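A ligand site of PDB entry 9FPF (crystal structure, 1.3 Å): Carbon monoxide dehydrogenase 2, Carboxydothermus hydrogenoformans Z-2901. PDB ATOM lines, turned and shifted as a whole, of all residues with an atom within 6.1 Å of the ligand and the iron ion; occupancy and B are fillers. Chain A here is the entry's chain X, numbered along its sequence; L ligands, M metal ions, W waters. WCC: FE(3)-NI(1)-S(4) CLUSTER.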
ATOM      1  N   HIS A  93       4.070  -2.205   8.824  1.00  0.00           N
ATOM      2  CA  HIS A  93       4.445  -2.894  10.053  1.00  0.00           C
ATOM      3  C   HIS A  93       4.649  -4.386   9.820  1.00  0.00           C
ATOM      4  O   HIS A  93       5.605  -4.977  10.347  1.00  0.00           O
ATOM      5  CB  HIS A  93       3.374  -2.670  11.126  1.00  0.00           C
ATOM      6  CG  HIS A  93       3.350  -1.286  11.705  1.00  0.00           C
ATOM      7  ND1 HIS A  93       2.168  -0.586  11.864  1.00  0.00           N
ATOM      8  CD2 HIS A  93       4.322  -0.493  12.194  1.00  0.00           C
ATOM      9  CE1 HIS A  93       2.424   0.581  12.412  1.00  0.00           C
ATOM     10  NE2 HIS A  93       3.725   0.669  12.622  1.00  0.00           N
ATOM     11  N   GLY A 260      15.133   4.974   9.581  1.00  0.00           N
ATOM     12  CA  GLY A 260      14.231   3.972   9.031  1.00  0.00           C
ATOM     13  C   GLY A 260      13.711   3.090  10.142  1.00  0.00           C
ATOM     14  O   GLY A 260      13.348   3.612  11.198  1.00  0.00           O
ATOM     15  N   HIS A 261      13.730   1.767   9.958  1.00  0.00           N
ATOM     16  CA  HIS A 261      12.925   0.935  10.847  1.00  0.00           C
ATOM     17  C   HIS A 261      13.535  -0.363  11.353  1.00  0.00           C
ATOM     18  O   HIS A 261      13.375  -0.679  12.544  1.00  0.00           O
ATOM     19  CB  HIS A 261      11.532   0.705  10.211  1.00  0.00           C
ATOM     20  CG  HIS A 261      10.652   1.882  10.443  1.00  0.00           C
ATOM     21  ND1 HIS A 261      10.788   3.040   9.723  1.00  0.00           N
ATOM     22  CD2 HIS A 261       9.757   2.148  11.430  1.00  0.00           C
ATOM     23  CE1 HIS A 261       9.976   3.956  10.211  1.00  0.00           C
ATOM     24  NE2 HIS A 261       9.360   3.449  11.264  1.00  0.00           N
ATOM     25  N   CYS A 294      14.429   8.448  14.092  1.00  0.00           N
ATOM     26  CA  CYS A 294      13.166   7.709  13.900  1.00  0.00           C
ATOM     27  C   CYS A 294      13.245   6.356  14.607  1.00  0.00           C
ATOM     28  O   CYS A 294      13.956   6.219  15.610  1.00  0.00           O
ATOM     29  CB  CYS A 294      12.790   7.667  12.431  1.00  0.00           C
ATOM     30  SG  CYS A 294      12.079   9.222  11.818  1.00  0.00           S
ATOM     31  N   CYS A 295      12.528   5.344  14.100  1.00  0.00           N
ATOM     32  CA  CYS A 295      12.304   4.128  14.885  1.00  0.00           C
ATOM     33  C   CYS A 295      13.542   3.240  14.945  1.00  0.00           C
ATOM     34  O   CYS A 295      13.823   2.621  15.981  1.00  0.00           O
ATOM     35  CB  CYS A 295      11.145   3.314  14.313  1.00  0.00           C
ATOM     36  SG  CYS A 295       9.519   3.785  14.921  1.00  0.00           S
ATOM     37  N   HIS A 311      14.121  13.138  15.227  1.00  0.00           N
ATOM     38  CA  HIS A 311      13.028  12.272  14.814  1.00  0.00           C
ATOM     39  C   HIS A 311      12.377  12.826  13.554  1.00  0.00           C
ATOM     40  O   HIS A 311      12.867  13.761  12.926  1.00  0.00           O
ATOM     41  CB  HIS A 311      12.068  12.062  15.992  1.00  0.00           C
ATOM     42  CG  HIS A 311      12.746  11.479  17.191  1.00  0.00           C
ATOM     43  ND1 HIS A 311      13.354  12.257  18.156  1.00  0.00           N
ATOM     44  CD2 HIS A 311      12.962  10.192  17.550  1.00  0.00           C
ATOM     45  CE1 HIS A 311      13.907  11.472  19.066  1.00  0.00           C
ATOM     46  NE2 HIS A 311      13.683  10.213  18.724  1.00  0.00           N
ATOM     47  N   SER A 312      11.354  12.108  13.121  1.00  0.00           N
ATOM     48  CA  SER A 312      10.257  12.549  12.270  1.00  0.00           C
ATOM     49  C   SER A 312      10.508  13.816  11.455  1.00  0.00           C
ATOM     50  O   SER A 312      11.370  13.841  10.572  1.00  0.00           O
ATOM     51  CB  SER A 312       9.020  12.663  13.174  1.00  0.00           C
ATOM     52  OG  SER A 312       7.783  12.682  12.457  1.00  0.00           O
ATOM     53  N   VAL A 313       9.727  14.861  11.741  1.00  0.00           N
ATOM     54  CA  VAL A 313       9.610  16.055  10.886  1.00  0.00           C
ATOM     55  C   VAL A 313      10.910  16.840  10.794  1.00  0.00           C
ATOM     56  O   VAL A 313      11.167  17.493   9.777  1.00  0.00           O
ATOM     57  CB  VAL A 313       8.421  16.942  11.355  1.00  0.00           C
ATOM     58  CG1 VAL A 313       8.747  17.622  12.676  1.00  0.00           C
ATOM     59  CG2 VAL A 313       8.082  17.994  10.296  1.00  0.00           C
ATOM     60  N   GLN A 332      10.687   3.413   5.441  1.00  0.00           N
ATOM     61  CA  GLN A 332       9.572   4.036   6.148  1.00  0.00           C
ATOM     62  C   GLN A 332       9.984   5.328   6.849  1.00  0.00           C
ATOM     63  O   GLN A 332      10.945   5.326   7.639  1.00  0.00           O
ATOM     64  CB  GLN A 332       8.887   3.091   7.149  1.00  0.00           C
ATOM     65  CG  GLN A 332       8.303   1.844   6.543  1.00  0.00           C
ATOM     66  CD  GLN A 332       7.939   0.810   7.614  1.00  0.00           C
ATOM     67  OE1 GLN A 332       7.789   1.124   8.786  1.00  0.00           O
ATOM     68  NE2 GLN A 332       7.812  -0.436   7.186  1.00  0.00           N
ATOM     69  N   CYS A 333       9.269   6.424   6.572  1.00  0.00           N
ATOM     70  CA  CYS A 333       9.321   7.692   7.303  1.00  0.00           C
ATOM     71  C   CYS A 333      10.564   8.504   6.974  1.00  0.00           C
ATOM     72  O   CYS A 333      10.851   9.484   7.680  1.00  0.00           O
ATOM     73  CB  CYS A 333       9.175   7.453   8.807  1.00  0.00           C
ATOM     74  SG  CYS A 333       7.616   6.640   9.177  1.00  0.00           S
ATOM     75  N   ALA A 444       1.830   7.988  21.151  1.00  0.00           N
ATOM     76  CA  ALA A 444       2.297   7.198  20.012  1.00  0.00           C
ATOM     77  C   ALA A 444       2.339   8.064  18.771  1.00  0.00           C
ATOM     78  O   ALA A 444       1.758   9.148  18.713  1.00  0.00           O
ATOM     79  CB  ALA A 444       1.377   5.997  19.796  1.00  0.00           C
ATOM     80  N   GLY A 445       3.042   7.550  17.767  1.00  0.00           N
ATOM     81  CA  GLY A 445       2.997   8.160  16.460  1.00  0.00           C
ATOM     82  C   GLY A 445       3.963   9.319  16.270  1.00  0.00           C
ATOM     83  O   GLY A 445       4.848   9.602  17.097  1.00  0.00           O
ATOM     84  N   CYS A 446       3.698  10.045  15.180  1.00  0.00           N
ATOM     85  CA  CYS A 446       4.643  10.911  14.484  1.00  0.00           C
ATOM     86  C   CYS A 446       4.614  12.347  15.021  1.00  0.00           C
ATOM     87  O   CYS A 446       3.816  12.710  15.877  1.00  0.00           O
ATOM     88  CB  CYS A 446       4.210  10.959  13.003  1.00  0.00           C
ATOM     89  SG  CYS A 446       3.489   9.377  12.358  1.00  0.00           S
ATOM     90  N   ASN A 447       5.483  13.195  14.452  1.00  0.00           N
ATOM     91  CA  ASN A 447       5.265  14.628  14.315  1.00  0.00           C
ATOM     92  C   ASN A 447       4.606  14.882  12.949  1.00  0.00           C
ATOM     93  O   ASN A 447       4.641  14.035  12.045  1.00  0.00           O
ATOM     94  CB  ASN A 447       6.586  15.429  14.357  1.00  0.00           C
ATOM     95  CG  ASN A 447       7.368  15.328  15.667  1.00  0.00           C
ATOM     96  OD1 ASN A 447       8.567  15.020  15.635  1.00  0.00           O
ATOM     97  ND2 ASN A 447       6.732  15.676  16.794  1.00  0.00           N
ATOM     98  N   THR A 474       5.977   5.733  22.785  1.00  0.00           N
ATOM     99  CA  THR A 474       6.715   5.029  21.748  1.00  0.00           C
ATOM    100  C   THR A 474       6.957   5.951  20.545  1.00  0.00           C
ATOM    101  O   THR A 474       6.377   7.028  20.414  1.00  0.00           O
ATOM    102  CB  THR A 474       5.917   3.828  21.232  1.00  0.00           C
ATOM    103  OG1 THR A 474       4.708   4.338  20.652  1.00  0.00           O
ATOM    104  CG2 THR A 474       5.617   2.813  22.322  1.00  0.00           C
ATOM    105  N   GLY A 475       7.830   5.490  19.645  1.00  0.00           N
ATOM    106  CA  GLY A 475       8.028   6.163  18.369  1.00  0.00           C
ATOM    107  C   GLY A 475       8.459   7.597  18.530  1.00  0.00           C
ATOM    108  O   GLY A 475       9.281   7.939  19.401  1.00  0.00           O
ATOM    109  N   CYS A 476       7.936   8.444  17.675  1.00  0.00           N
ATOM    110  CA  CYS A 476       8.312   9.848  17.726  1.00  0.00           C
ATOM    111  C   CYS A 476       7.513  10.627  18.784  1.00  0.00           C
ATOM    112  O   CYS A 476       7.833  11.794  19.045  1.00  0.00           O
ATOM    113  CB  CYS A 476       8.297  10.413  16.287  1.00  0.00           C
ATOM    114  SG  CYS A 476       9.434   9.521  15.084  1.00  0.00           S
ATOM    115  N   GLY A 477       6.548   9.993  19.459  1.00  0.00           N
ATOM    116  CA  GLY A 477       6.015  10.564  20.673  1.00  0.00           C
ATOM    117  C   GLY A 477       7.012  10.429  21.806  1.00  0.00           C
ATOM    118  O   GLY A 477       7.262  11.380  22.557  1.00  0.00           O
ATOM    119  N   SER A 525       9.933   1.493  19.917  1.00  0.00           N
ATOM    120  CA  SER A 525       9.640   1.896  18.557  1.00  0.00           C
ATOM    121  C   SER A 525       8.147   1.814  18.292  1.00  0.00           C
ATOM    122  O   SER A 525       7.340   1.400  19.125  1.00  0.00           O
ATOM    123  CB  SER A 525      10.330   0.938  17.606  1.00  0.00           C
ATOM    124  OG  SER A 525       9.797  -0.355  17.826  1.00  0.00           O
ATOM    125  N   CYS A 526       7.770   2.177  17.070  1.00  0.00           N
ATOM    126  CA  CYS A 526       6.295   2.025  16.671  1.00  0.00           C
ATOM    127  C   CYS A 526       5.717   0.553  16.711  1.00  0.00           C
ATOM    128  O   CYS A 526       4.570   0.225  17.212  1.00  0.00           O
ATOM    129  CB  CYS A 526       6.008   2.676  15.329  1.00  0.00           C
ATOM    130  SG  CYS A 526       6.249   4.505  15.439  1.00  0.00           S
ATOM    131  N   MET A 560       0.957  11.404  11.474  1.00  0.00           N
ATOM    132  CA  MET A 560       1.275  11.631  10.063  1.00  0.00           C
ATOM    133  C   MET A 560       1.112  10.384   9.174  1.00  0.00           C
ATOM    134  O   MET A 560       0.367  10.402   8.189  1.00  0.00           O
ATOM    135  CB  MET A 560       2.696  12.185   9.942  1.00  0.00           C
ATOM    136  CG  MET A 560       3.202  12.460   8.545  1.00  0.00           C
ATOM    137  SD  MET A 560       4.096  11.111   7.746  1.00  0.00           S
ATOM    138  CE  MET A 560       5.499  10.867   8.865  1.00  0.00           C
ATOM    139  N   HIS A 561       1.796   9.296   9.513  1.00  0.00           N
ATOM    140  CA  HIS A 561       1.933   8.190   8.566  1.00  0.00           C
ATOM    141  C   HIS A 561       0.679   7.325   8.547  1.00  0.00           C
ATOM    142  O   HIS A 561      -0.087   7.258   9.513  1.00  0.00           O
ATOM    143  CB  HIS A 561       3.160   7.350   8.979  1.00  0.00           C
ATOM    144  CG  HIS A 561       3.723   6.505   7.871  1.00  0.00           C
ATOM    145  ND1 HIS A 561       3.187   5.285   7.512  1.00  0.00           N
ATOM    146  CD2 HIS A 561       4.776   6.703   7.048  1.00  0.00           C
ATOM    147  CE1 HIS A 561       3.884   4.774   6.527  1.00  0.00           C
ATOM    148  NE2 HIS A 561       4.848   5.630   6.213  1.00  0.00           N
ATOM    149  N   LYS A 563       0.833   4.282   8.889  1.00  0.00           N
ATOM    150  CA  LYS A 563       1.040   3.384  10.018  1.00  0.00           C
ATOM    151  C   LYS A 563       0.402   3.915  11.298  1.00  0.00           C
ATOM    152  O   LYS A 563      -0.086   3.133  12.128  1.00  0.00           O
ATOM    153  CB  LYS A 563       2.545   3.176  10.247  1.00  0.00           C
ATOM    154  CG  LYS A 563       3.233   2.254   9.269  1.00  0.00           C
ATOM    155  CD  LYS A 563       4.740   2.150   9.492  1.00  0.00           C
ATOM    156  CE  LYS A 563       5.496   3.398   9.078  1.00  0.00           C
ATOM    157  NZ  LYS A 563       6.787   3.461   9.822  1.00  0.00           N
ATOM    158  N   ALA A 564       0.422   5.240  11.495  1.00  0.00           N
ATOM    159  CA  ALA A 564      -0.175   5.807  12.709  1.00  0.00           C
ATOM    160  C   ALA A 564      -1.693   5.730  12.670  1.00  0.00           C
ATOM    161  O   ALA A 564      -2.338   5.541  13.717  1.00  0.00           O
ATOM    162  CB  ALA A 564       0.314   7.248  12.890  1.00  0.00           C
ATOM    163  N   ILE A 567      -2.402   2.109  13.692  1.00  0.00           N
ATOM    164  CA  ILE A 567      -2.232   1.951  15.143  1.00  0.00           C
ATOM    165  C   ILE A 567      -3.398   2.586  15.904  1.00  0.00           C
ATOM    166  O   ILE A 567      -3.960   1.988  16.830  1.00  0.00           O
ATOM    167  CB  ILE A 567      -0.878   2.529  15.593  1.00  0.00           C
ATOM    168  CG1 ILE A 567       0.282   1.658  15.132  1.00  0.00           C
ATOM    169  CG2 ILE A 567      -0.834   2.677  17.124  1.00  0.00           C
ATOM    170  CD1 ILE A 567       1.654   2.366  15.131  1.00  0.00           C
HETATM  171 NI   WCC L   1       5.882   5.673  13.732  1.00  0.00          NI
HETATM  172 FE1  WCC L   1       7.392   7.151  11.351  1.00  0.00          FE
HETATM  173 FE3  WCC L   1       5.466   8.120  12.719  1.00  0.00          FE
HETATM  174 FE4  WCC L   1       7.973   8.402  13.644  1.00  0.00          FE
HETATM  175  S1  WCC L   1       6.191   7.612  14.778  1.00  0.00           S
HETATM  176  S2  WCC L   1       7.169   9.455  11.698  1.00  0.00           S
HETATM  177  S3  WCC L   1       9.224   6.751  12.683  1.00  0.00           S
HETATM  178  S4  WCC L   1       5.349   6.135  11.693  1.00  0.00           S
HETATM  179 FE    FE M   1       8.376   4.497  12.890  1.00  0.00          FE
HETATM  180  O   HOH W   1       6.738   3.502  12.470  1.00  0.00           O
HETATM  181  O   HOH W   2       9.117  10.963   9.238  1.00  0.00           O
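FE1 of the ligand is bound by SG of Cys 333, 2.2 Å away. The backbone NH of Cys 476 lies close to a sulfur (S1) of the ligand, 3.5 Å away. FE3 of the ligand is bound by SG of Cys 446, 2.4 Å away. The side-chain sulfur of Cys 526 binds a nickel atom (NI) of the ligand, 2.1 Å away. NZ of Lys 563 sits close to S4 of the ligand. A sulfur (S2) of the ligand sits close to the side-chain hydroxyl (OG) of Ser 312, 3.4 Å away. The backbone NH (N) of Cys 446 lies close to a sulfur (S1) of the ligand (3.5 Å). The side-chain sulfur of Cys 476 is bound to an iron atom (FE4) of the ligand, at 2.3 Å.
The backbone NH of Cys 476 sits close to the backbone carbonyl oxygen of Gly 445 (3.3 Å). A ring nitrogen (NE2) of His 261 lies close to the side-chain amino group of Lys 563, 2.9 Å away. SG of Cys 295 sits close to N of Cys 526 (3.2 Å). A ring nitrogen (ND1) of His 561 is in hydrogen-bond range of the backbone NH of Lys 563 (2.9 Å). The side-chain sulfur of Cys 446 lies close to the backbone NH of Met 560 (3.4 Å). SG of Cys 294 sits at hydrogen-bond distance from N of Ser 312, at 3.2 Å. The backbone NH (N) of Ser 312 sits close to the side-chain sulfur (SG) of Cys 476 (3.8 Å). O of Gly 445 lies within hydrogen-bond range of N of Gly 477 (2.9 Å).
A sulfur (S1) of the ligand lies close to the backbone carbonyl oxygen (O) of Gly 445 (3.3 Å). Merely in contact with the ligand: Met 560 (3.6 Å), Cys 294 (3.7 Å) and His 561 (3.7 Å). Hydrophobic or aromatic side chains that line the ligand: His 261, Met 560 and His 561. The nearest printed residue that does not touch the ligand is Gly 475 (4.3 Å).
Cys 526 touches the iron ion. Lys 563 touches the iron ion. Within 4 Å of the iron ion: His 261, Cys 295, Cys 526 and Lys 563. The nearest printed residue that does not touch the iron ion is Cys 333 (4.4 Å).
The iron ion is bound by water W1 (2.0 Å), a ring nitrogen (NE2) of His 261 (2.2 Å), a sulfur (S3) of the ligand (2.4 Å) and the side-chain sulfur (SG) of Cys 295 (2.4 Å). The iron ion has four donor atoms within binding distance.
Water W2 bridges the backbone carbonyl oxygen (O) of Cys 333 (2.8 Å) and a sulfur (S2) of the ligand (3.5 Å).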
